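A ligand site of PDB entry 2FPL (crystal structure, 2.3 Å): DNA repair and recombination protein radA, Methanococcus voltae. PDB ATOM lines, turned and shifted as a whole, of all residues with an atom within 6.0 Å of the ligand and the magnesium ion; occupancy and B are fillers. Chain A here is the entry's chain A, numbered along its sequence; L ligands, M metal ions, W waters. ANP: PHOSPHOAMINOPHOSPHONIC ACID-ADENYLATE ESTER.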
ATOM      1  N   GLY A 105     -28.175  -7.874 -11.105  1.00  0.00           N
ATOM      2  CA  GLY A 105     -26.923  -7.198 -10.824  1.00  0.00           C
ATOM      3  C   GLY A 105     -26.867  -5.827 -11.452  1.00  0.00           C
ATOM      4  O   GLY A 105     -27.641  -5.498 -12.357  1.00  0.00           O
ATOM      5  N   VAL A 106     -25.927  -5.021 -10.964  1.00  0.00           N
ATOM      6  CA  VAL A 106     -25.748  -3.677 -11.462  1.00  0.00           C
ATOM      7  C   VAL A 106     -25.083  -3.713 -12.823  1.00  0.00           C
ATOM      8  O   VAL A 106     -24.510  -4.733 -13.221  1.00  0.00           O
ATOM      9  CB  VAL A 106     -24.887  -2.843 -10.500  1.00  0.00           C
ATOM     10  CG1 VAL A 106     -25.580  -2.722  -9.157  1.00  0.00           C
ATOM     11  CG2 VAL A 106     -23.525  -3.497 -10.325  1.00  0.00           C
ATOM     12  N   PHE A 107     -25.149  -2.588 -13.525  1.00  0.00           N
ATOM     13  CA  PHE A 107     -24.539  -2.467 -14.838  1.00  0.00           C
ATOM     14  C   PHE A 107     -23.118  -2.998 -14.804  1.00  0.00           C
ATOM     15  O   PHE A 107     -22.340  -2.647 -13.916  1.00  0.00           O
ATOM     16  CB  PHE A 107     -24.515  -1.000 -15.268  1.00  0.00           C
ATOM     17  CG  PHE A 107     -25.860  -0.437 -15.634  1.00  0.00           C
ATOM     18  CD1 PHE A 107     -26.527  -0.876 -16.783  1.00  0.00           C
ATOM     19  CD2 PHE A 107     -26.477   0.529 -14.835  1.00  0.00           C
ATOM     20  CE1 PHE A 107     -27.785  -0.359 -17.130  1.00  0.00           C
ATOM     21  CE2 PHE A 107     -27.728   1.051 -15.170  1.00  0.00           C
ATOM     22  CZ  PHE A 107     -28.380   0.607 -16.327  1.00  0.00           C
ATOM     23  N   GLY A 108     -22.785  -3.851 -15.767  1.00  0.00           N
ATOM     24  CA  GLY A 108     -21.449  -4.404 -15.874  1.00  0.00           C
ATOM     25  C   GLY A 108     -21.027  -5.409 -14.821  1.00  0.00           C
ATOM     26  O   GLY A 108     -19.858  -5.781 -14.782  1.00  0.00           O
ATOM     27  N   SER A 109     -21.961  -5.863 -13.993  1.00  0.00           N
ATOM     28  CA  SER A 109     -21.621  -6.831 -12.959  1.00  0.00           C
ATOM     29  C   SER A 109     -21.243  -8.212 -13.465  1.00  0.00           C
ATOM     30  O   SER A 109     -20.652  -8.993 -12.727  1.00  0.00           O
ATOM     31  CB  SER A 109     -22.761  -6.936 -11.933  1.00  0.00           C
ATOM     32  OG  SER A 109     -24.006  -7.168 -12.554  1.00  0.00           O
ATOM     33  N   GLY A 110     -21.577  -8.525 -14.719  1.00  0.00           N
ATOM     34  CA  GLY A 110     -21.236  -9.830 -15.286  1.00  0.00           C
ATOM     35  C   GLY A 110     -22.389 -10.750 -15.675  1.00  0.00           C
ATOM     36  O   GLY A 110     -22.186 -11.918 -16.018  1.00  0.00           O
ATOM     37  N   LYS A 111     -23.610 -10.224 -15.615  1.00  0.00           N
ATOM     38  CA  LYS A 111     -24.801 -11.000 -15.952  1.00  0.00           C
ATOM     39  C   LYS A 111     -24.619 -11.774 -17.255  1.00  0.00           C
ATOM     40  O   LYS A 111     -24.770 -12.999 -17.294  1.00  0.00           O
ATOM     41  CB  LYS A 111     -26.009 -10.065 -16.068  1.00  0.00           C
ATOM     42  CG  LYS A 111     -26.318  -9.299 -14.792  1.00  0.00           C
ATOM     43  CD  LYS A 111     -27.560  -8.417 -14.945  1.00  0.00           C
ATOM     44  CE  LYS A 111     -27.303  -7.230 -15.875  1.00  0.00           C
ATOM     45  NZ  LYS A 111     -26.292  -6.280 -15.312  1.00  0.00           N
ATOM     46  N   THR A 112     -24.296 -11.049 -18.319  1.00  0.00           N
ATOM     47  CA  THR A 112     -24.115 -11.658 -19.633  1.00  0.00           C
ATOM     48  C   THR A 112     -22.945 -12.661 -19.659  1.00  0.00           C
ATOM     49  O   THR A 112     -23.041 -13.686 -20.332  1.00  0.00           O
ATOM     50  CB  THR A 112     -23.930 -10.565 -20.700  1.00  0.00           C
ATOM     51  OG1 THR A 112     -25.106  -9.736 -20.715  1.00  0.00           O
ATOM     52  CG2 THR A 112     -23.734 -11.175 -22.083  1.00  0.00           C
ATOM     53  N   GLN A 113     -21.873 -12.377 -18.932  1.00  0.00           N
ATOM     54  CA  GLN A 113     -20.737 -13.290 -18.904  1.00  0.00           C
ATOM     55  C   GLN A 113     -21.167 -14.650 -18.367  1.00  0.00           C
ATOM     56  O   GLN A 113     -20.811 -15.692 -18.933  1.00  0.00           O
ATOM     57  CB  GLN A 113     -19.600 -12.746 -18.023  1.00  0.00           C
ATOM     58  CG  GLN A 113     -18.913 -11.487 -18.565  1.00  0.00           C
ATOM     59  CD  GLN A 113     -18.501 -11.634 -20.030  1.00  0.00           C
ATOM     60  OE1 GLN A 113     -17.515 -12.312 -20.343  1.00  0.00           O
ATOM     61  NE2 GLN A 113     -19.261 -11.019 -20.925  1.00  0.00           N
ATOM     62  N   ILE A 114     -21.930 -14.647 -17.282  1.00  0.00           N
ATOM     63  CA  ILE A 114     -22.389 -15.889 -16.671  1.00  0.00           C
ATOM     64  C   ILE A 114     -23.252 -16.691 -17.643  1.00  0.00           C
ATOM     65  O   ILE A 114     -23.171 -17.927 -17.674  1.00  0.00           O
ATOM     66  CB  ILE A 114     -23.157 -15.584 -15.355  1.00  0.00           C
ATOM     67  CG1 ILE A 114     -22.203 -14.903 -14.362  1.00  0.00           C
ATOM     68  CG2 ILE A 114     -23.725 -16.857 -14.746  1.00  0.00           C
ATOM     69  CD1 ILE A 114     -22.872 -14.389 -13.099  1.00  0.00           C
ATOM     70  N   GLU A 151     -30.824  -8.040 -25.341  1.00  0.00           N
ATOM     71  CA  GLU A 151     -29.949  -6.871 -25.310  1.00  0.00           C
ATOM     72  C   GLU A 151     -29.128  -6.689 -26.579  1.00  0.00           C
ATOM     73  O   GLU A 151     -28.746  -5.564 -26.919  1.00  0.00           O
ATOM     74  CB  GLU A 151     -29.005  -6.998 -24.126  1.00  0.00           C
ATOM     75  CG  GLU A 151     -29.700  -7.315 -22.808  1.00  0.00           C
ATOM     76  CD  GLU A 151     -30.609  -6.202 -22.330  1.00  0.00           C
ATOM     77  OE1 GLU A 151     -30.424  -5.759 -21.170  1.00  0.00           O
ATOM     78  OE2 GLU A 151     -31.494  -5.777 -23.096  1.00  0.00           O
ATOM     79  N   THR A 153     -26.302  -8.510 -26.957  1.00  0.00           N
ATOM     80  CA  THR A 153     -24.935  -8.683 -26.489  1.00  0.00           C
ATOM     81  C   THR A 153     -24.405 -10.111 -26.575  1.00  0.00           C
ATOM     82  O   THR A 153     -23.470 -10.475 -25.870  1.00  0.00           O
ATOM     83  CB  THR A 153     -24.779  -8.166 -25.040  1.00  0.00           C
ATOM     84  OG1 THR A 153     -25.913  -8.587 -24.265  1.00  0.00           O
ATOM     85  CG2 THR A 153     -24.674  -6.641 -25.015  1.00  0.00           C
ATOM     86  N   ARG A 158     -16.639 -14.419 -27.567  1.00  0.00           N
ATOM     87  CA  ARG A 158     -16.533 -14.719 -26.150  1.00  0.00           C
ATOM     88  C   ARG A 158     -16.751 -16.222 -25.904  1.00  0.00           C
ATOM     89  O   ARG A 158     -16.123 -16.814 -25.027  1.00  0.00           O
ATOM     90  CB  ARG A 158     -17.537 -13.885 -25.362  1.00  0.00           C
ATOM     91  CG  ARG A 158     -17.298 -13.868 -23.869  1.00  0.00           C
ATOM     92  CD  ARG A 158     -15.906 -13.362 -23.516  1.00  0.00           C
ATOM     93  NE  ARG A 158     -15.741 -13.288 -22.081  1.00  0.00           N
ATOM     94  CZ  ARG A 158     -14.612 -13.564 -21.427  1.00  0.00           C
ATOM     95  NH1 ARG A 158     -14.572 -13.462 -20.111  1.00  0.00           N
ATOM     96  NH2 ARG A 158     -13.532 -13.938 -22.103  1.00  0.00           N
ATOM     97  N   GLN A 161     -13.519 -18.040 -26.982  1.00  0.00           N
ATOM     98  CA  GLN A 161     -12.498 -17.763 -25.990  1.00  0.00           C
ATOM     99  C   GLN A 161     -12.718 -18.558 -24.709  1.00  0.00           C
ATOM    100  O   GLN A 161     -11.830 -19.295 -24.245  1.00  0.00           O
ATOM    101  CB  GLN A 161     -12.483 -16.253 -25.718  1.00  0.00           C
ATOM    102  CG  GLN A 161     -11.443 -15.787 -24.724  1.00  0.00           C
ATOM    103  CD  GLN A 161     -11.375 -14.262 -24.635  1.00  0.00           C
ATOM    104  OE1 GLN A 161     -12.407 -13.586 -24.535  1.00  0.00           O
ATOM    105  NE2 GLN A 161     -10.174 -13.722 -24.650  1.00  0.00           N
ATOM    106  N   ASP A 211     -31.499 -13.311 -21.509  1.00  0.00           N
ATOM    107  CA  ASP A 211     -30.694 -12.143 -21.197  1.00  0.00           C
ATOM    108  C   ASP A 211     -31.097 -11.031 -22.164  1.00  0.00           C
ATOM    109  O   ASP A 211     -30.729 -11.077 -23.333  1.00  0.00           O
ATOM    110  CB  ASP A 211     -29.208 -12.498 -21.356  1.00  0.00           C
ATOM    111  CG  ASP A 211     -28.272 -11.344 -21.036  1.00  0.00           C
ATOM    112  OD1 ASP A 211     -28.538 -10.573 -20.089  1.00  0.00           O
ATOM    113  OD2 ASP A 211     -27.241 -11.208 -21.727  1.00  0.00           O
ATOM    114  N   GLN A 257     -31.346  -6.463 -14.651  1.00  0.00           N
ATOM    115  CA  GLN A 257     -30.582  -5.259 -14.338  1.00  0.00           C
ATOM    116  C   GLN A 257     -31.206  -4.500 -13.170  1.00  0.00           C
ATOM    117  O   GLN A 257     -32.350  -4.075 -13.236  1.00  0.00           O
ATOM    118  CB  GLN A 257     -30.505  -4.359 -15.569  1.00  0.00           C
ATOM    119  CG  GLN A 257     -30.201  -2.896 -15.254  1.00  0.00           C
ATOM    120  CD  GLN A 257     -28.855  -2.714 -14.611  1.00  0.00           C
ATOM    121  OE1 GLN A 257     -28.685  -1.884 -13.715  1.00  0.00           O
ATOM    122  NE2 GLN A 257     -27.876  -3.478 -15.068  1.00  0.00           N
ATOM    123  N   LYS A 290     -19.621  -5.759  -8.525  1.00  0.00           N
ATOM    124  CA  LYS A 290     -18.193  -5.779  -8.833  1.00  0.00           C
ATOM    125  C   LYS A 290     -17.363  -5.640  -7.573  1.00  0.00           C
ATOM    126  O   LYS A 290     -17.706  -4.877  -6.673  1.00  0.00           O
ATOM    127  CB  LYS A 290     -17.812  -4.633  -9.767  1.00  0.00           C
ATOM    128  CG  LYS A 290     -18.347  -4.704 -11.179  1.00  0.00           C
ATOM    129  CD  LYS A 290     -17.769  -3.550 -11.989  1.00  0.00           C
ATOM    130  CE  LYS A 290     -18.446  -3.369 -13.332  1.00  0.00           C
ATOM    131  NZ  LYS A 290     -17.984  -2.150 -14.065  1.00  0.00           N
ATOM    132  N   ARG A 296     -15.797 -10.317  -8.352  1.00  0.00           N
ATOM    133  CA  ARG A 296     -17.248 -10.234  -8.468  1.00  0.00           C
ATOM    134  C   ARG A 296     -17.820 -10.902  -7.223  1.00  0.00           C
ATOM    135  O   ARG A 296     -17.339 -11.935  -6.771  1.00  0.00           O
ATOM    136  CB  ARG A 296     -17.731 -10.975  -9.719  1.00  0.00           C
ATOM    137  CG  ARG A 296     -17.200 -10.388 -11.013  1.00  0.00           C
ATOM    138  CD  ARG A 296     -17.770  -8.995 -11.253  1.00  0.00           C
ATOM    139  NE  ARG A 296     -17.368  -8.483 -12.563  1.00  0.00           N
ATOM    140  CZ  ARG A 296     -16.181  -7.946 -12.837  1.00  0.00           C
ATOM    141  NH1 ARG A 296     -15.265  -7.833 -11.876  1.00  0.00           N
ATOM    142  NH2 ARG A 296     -15.903  -7.539 -14.061  1.00  0.00           N
ATOM    143  N   ILE A 315     -13.936 -12.611 -13.236  1.00  0.00           N
ATOM    144  CA  ILE A 315     -14.165 -12.770 -14.653  1.00  0.00           C
ATOM    145  C   ILE A 315     -12.893 -12.318 -15.348  1.00  0.00           C
ATOM    146  O   ILE A 315     -12.476 -11.158 -15.231  1.00  0.00           O
ATOM    147  CB  ILE A 315     -15.375 -11.932 -15.126  1.00  0.00           C
ATOM    148  CG1 ILE A 315     -16.624 -12.352 -14.344  1.00  0.00           C
ATOM    149  CG2 ILE A 315     -15.592 -12.128 -16.622  1.00  0.00           C
ATOM    150  CD1 ILE A 315     -17.895 -11.576 -14.707  1.00  0.00           C
ATOM    151  N   THR A 316     -12.268 -13.247 -16.053  1.00  0.00           N
ATOM    152  CA  THR A 316     -11.027 -12.978 -16.762  1.00  0.00           C
ATOM    153  C   THR A 316     -11.260 -13.366 -18.208  1.00  0.00           C
ATOM    154  O   THR A 316     -12.401 -13.601 -18.613  1.00  0.00           O
ATOM    155  CB  THR A 316      -9.907 -13.828 -16.207  1.00  0.00           C
ATOM    156  OG1 THR A 316     -10.188 -15.202 -16.517  1.00  0.00           O
ATOM    157  CG2 THR A 316      -9.798 -13.672 -14.702  1.00  0.00           C
ATOM    158  N   GLU A 317     -10.179 -13.472 -18.989  1.00  0.00           N
ATOM    159  CA  GLU A 317     -10.298 -13.855 -20.390  1.00  0.00           C
ATOM    160  C   GLU A 317     -10.840 -15.274 -20.490  1.00  0.00           C
ATOM    161  O   GLU A 317     -11.420 -15.645 -21.510  1.00  0.00           O
ATOM    162  CB  GLU A 317      -8.934 -13.807 -21.102  1.00  0.00           C
ATOM    163  CG  GLU A 317      -7.772 -13.290 -20.277  1.00  0.00           C
ATOM    164  CD  GLU A 317      -7.237 -14.314 -19.281  1.00  0.00           C
ATOM    165  OE1 GLU A 317      -6.792 -15.409 -19.706  1.00  0.00           O
ATOM    166  OE2 GLU A 317      -7.242 -14.012 -18.069  1.00  0.00           O
ATOM    167  N   LYS A 318     -10.651 -16.044 -19.429  1.00  0.00           N
ATOM    168  CA  LYS A 318     -11.110 -17.422 -19.419  1.00  0.00           C
ATOM    169  C   LYS A 318     -12.579 -17.571 -19.056  1.00  0.00           C
ATOM    170  O   LYS A 318     -13.162 -18.645 -19.189  1.00  0.00           O
ATOM    171  CB  LYS A 318     -10.255 -18.238 -18.440  1.00  0.00           C
ATOM    172  CG  LYS A 318      -8.770 -18.115 -18.707  1.00  0.00           C
ATOM    173  CD  LYS A 318      -7.961 -18.931 -17.727  1.00  0.00           C
ATOM    174  CE  LYS A 318      -6.480 -18.628 -17.864  1.00  0.00           C
ATOM    175  NZ  LYS A 318      -5.690 -19.471 -16.940  1.00  0.00           N
HETATM  176  PG  ANP L   1     -25.069  -4.940 -18.574  1.00  0.00           P
HETATM  177  O1G ANP L   1     -25.863  -4.622 -17.438  1.00  0.00           O
HETATM  178  O2G ANP L   1     -25.789  -5.908 -19.453  1.00  0.00           O
HETATM  179  O3G ANP L   1     -24.806  -3.728 -19.319  1.00  0.00           O
HETATM  180  PB  ANP L   1     -23.454  -7.068 -17.530  1.00  0.00           P
HETATM  181  O1B ANP L   1     -24.133  -8.050 -18.410  1.00  0.00           O
HETATM  182  O2B ANP L   1     -23.964  -7.158 -16.175  1.00  0.00           O
HETATM  183  N3B ANP L   1     -23.602  -5.596 -18.079  1.00  0.00           N
HETATM  184  PA  ANP L   1     -21.109  -8.168 -18.653  1.00  0.00           P
HETATM  185  O1A ANP L   1     -21.616  -9.614 -18.744  1.00  0.00           O
HETATM  186  O2A ANP L   1     -21.325  -7.481 -19.934  1.00  0.00           O
HETATM  187  O3A ANP L   1     -21.879  -7.399 -17.466  1.00  0.00           O
HETATM  188  O5' ANP L   1     -19.506  -8.205 -18.279  1.00  0.00           O
HETATM  189  C5' ANP L   1     -18.561  -7.154 -18.795  1.00  0.00           C
HETATM  190  C4' ANP L   1     -17.375  -7.360 -18.253  1.00  0.00           C
HETATM  191  O4' ANP L   1     -16.902  -8.705 -18.648  1.00  0.00           O
HETATM  192  C3' ANP L   1     -16.303  -6.427 -18.873  1.00  0.00           C
HETATM  193  O3' ANP L   1     -16.436  -5.073 -18.661  1.00  0.00           O
HETATM  194  C2' ANP L   1     -14.981  -7.234 -18.796  1.00  0.00           C
HETATM  195  O2' ANP L   1     -14.328  -6.892 -17.454  1.00  0.00           O
HETATM  196  C1' ANP L   1     -15.453  -8.701 -18.727  1.00  0.00           C
HETATM  197  N9  ANP L   1     -15.096  -9.234 -19.923  1.00  0.00           N
HETATM  198  C8  ANP L   1     -15.907  -9.363 -21.077  1.00  0.00           C
HETATM  199  N7  ANP L   1     -15.233  -9.906 -22.021  1.00  0.00           N
HETATM  200  C5  ANP L   1     -13.983 -10.150 -21.587  1.00  0.00           C
HETATM  201  C6  ANP L   1     -12.867 -10.706 -22.161  1.00  0.00           C
HETATM  202  N6  ANP L   1     -12.892 -11.120 -23.450  1.00  0.00           N
HETATM  203  N1  ANP L   1     -11.691 -10.825 -21.397  1.00  0.00           N
HETATM  204  C2  ANP L   1     -11.642 -10.392 -20.052  1.00  0.00           C
HETATM  205  N3  ANP L   1     -12.727  -9.841 -19.451  1.00  0.00           N
HETATM  206  C4  ANP L   1     -13.893  -9.744 -20.264  1.00  0.00           C
HETATM  207 MG    MG M   1     -25.387  -7.742 -20.021  1.00  0.00          MG
HETATM  208  O   HOH W   1     -23.725  -7.209 -21.257  1.00  0.00           O
HETATM  209  O   HOH W   2     -20.923  -9.212 -21.955  1.00  0.00           O
HETATM  210  O   HOH W   3     -27.565  -4.943 -21.622  1.00  0.00           O
HETATM  211  O   HOH W   4     -23.206  -1.838 -18.057  1.00  0.00           O
HETATM  212  O   HOH W   5     -24.166  -4.519 -21.913  1.00  0.00           O
HETATM  213  O   HOH W   6     -29.066  -6.482 -18.837  1.00  0.00           O
HETATM  214  O   HOH W   7     -26.458  -7.266 -21.820  1.00  0.00           O
HETATM  215  O   HOH W   8     -18.678  -7.868 -15.468  1.00  0.00           O
HETATM  216  O   HOH W   9     -27.242  -8.397 -19.152  1.00  0.00           O
HETATM  217  O   HOH W  10     -17.823  -4.232 -16.103  1.00  0.00           O
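Water W2 bridges the side-chain amide nitrogen (NE2) of Gln 113 (2.7 Å) and an oxygen (O2A) of the ligand (2.7 Å).
Water W4 bridges an oxygen (O3G) of the ligand and the backbone NH (N) of Gly 108.
Water W8 lies within hydrogen-bond range of O of Gly 108, O5' of the ligand, N of Gly 110 and NH2 of Arg 296.
Water W10 lies within hydrogen-bond range of O of Gly 108 (2.9 Å), NZ of Lys 290 (2.9 Å) and O3' of the ligand (3.0 Å).
Within 4 Å of the magnesium ion: Thr 112.
N3B of the ligand lies close to N of Gly 108, at 3.0 Å.
Merely in contact with the ligand: Glu 317 (3.5 Å), Thr 316 (3.5 Å), Phe 107 (3.6 Å), Arg 296 (3.8 Å) and Val 106 (3.9 Å).
Hydrophobic or aromatic side chains that line the ligand: Phe 107.
14 residues have an atom within 4 Å of the ligand: Val 106, Phe 107, Gly 108, Ser 109, Gly 110, Lys 111, Thr 112, Gln 113, Arg 158, Gln 161, Gln 257, Arg 296, Thr 316 and Glu 317.
The nearest printed residue that does not touch the ligand is Ile 315 (4.02 Å).
The side-chain amide nitrogen (NE2) of Gln 257 sits close to the side-chain amino group (NZ) of Lys 111, at 3.2 Å.
OE1 of Gln 113 lies within hydrogen-bond range of NE of Arg 158 (2.7 Å).
The backbone carbonyl oxygen of Glu 317 is in hydrogen-bond range of the guanidinium group of Arg 158 (2.8 Å).
The guanidinium group (NH1) of Arg 158 sits at hydrogen-bond distance from the backbone carbonyl oxygen (O) of Thr 316, at 2.6 Å.
O of Ser 109 lies close to NE of Arg 296 (3.3 Å).
The backbone carbonyl oxygen (O) of Val 106 sits at hydrogen-bond distance from the side-chain hydroxyl (OG) of Ser 109, at 2.6 Å.
N of Phe 107 sits close to NE2 of Gln 257 (3.3 Å).
The backbone carbonyl oxygen (O) of Gly 105 sits at hydrogen-bond distance from the side-chain amide nitrogen (NE2) of Gln 257, at 3.4 Å.
An oxygen (O1A) of the ligand sits at hydrogen-bond distance from the backbone NH (N) of Thr 112 (3.1 Å).
The backbone NH (N) of Lys 111 is in hydrogen-bond range of an oxygen (O2B) of the ligand (3.1 Å).
The side-chain amino group (NZ) of Lys 111 lies within salt-bridge range of an oxygen (O2B) of the ligand, 2.6 Å away.
A nitrogen (N6) of the ligand lies within hydrogen-bond range of the side-chain amide oxygen (OE1) of Gln 161.
O1A of the ligand is in hydrogen-bond range of N of Gln 113, 2.8 Å away.
O3A of the ligand sits at hydrogen-bond distance from N of Gly 110 (3.0 Å).
The guanidinium group (NE) of Arg 158 lies within hydrogen-bond range of a nitrogen (N7) of the ligand.
The backbone NH (N) of Ser 109 is in hydrogen-bond range of an oxygen (O2B) of the ligand, 3.2 Å away.
NE2 of Gln 257 lies within hydrogen-bond range of O1G of the ligand (3.3 Å).
The magnesium ion is bound by an oxygen (O2G) of the ligand (2.0 Å), an oxygen (O1B) of the ligand (2.1 Å), the side-chain hydroxyl of Thr 112 (2.1 Å), water W1 (2.1 Å), water W7 (2.1 Å) and water W9 (2.2 Å).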
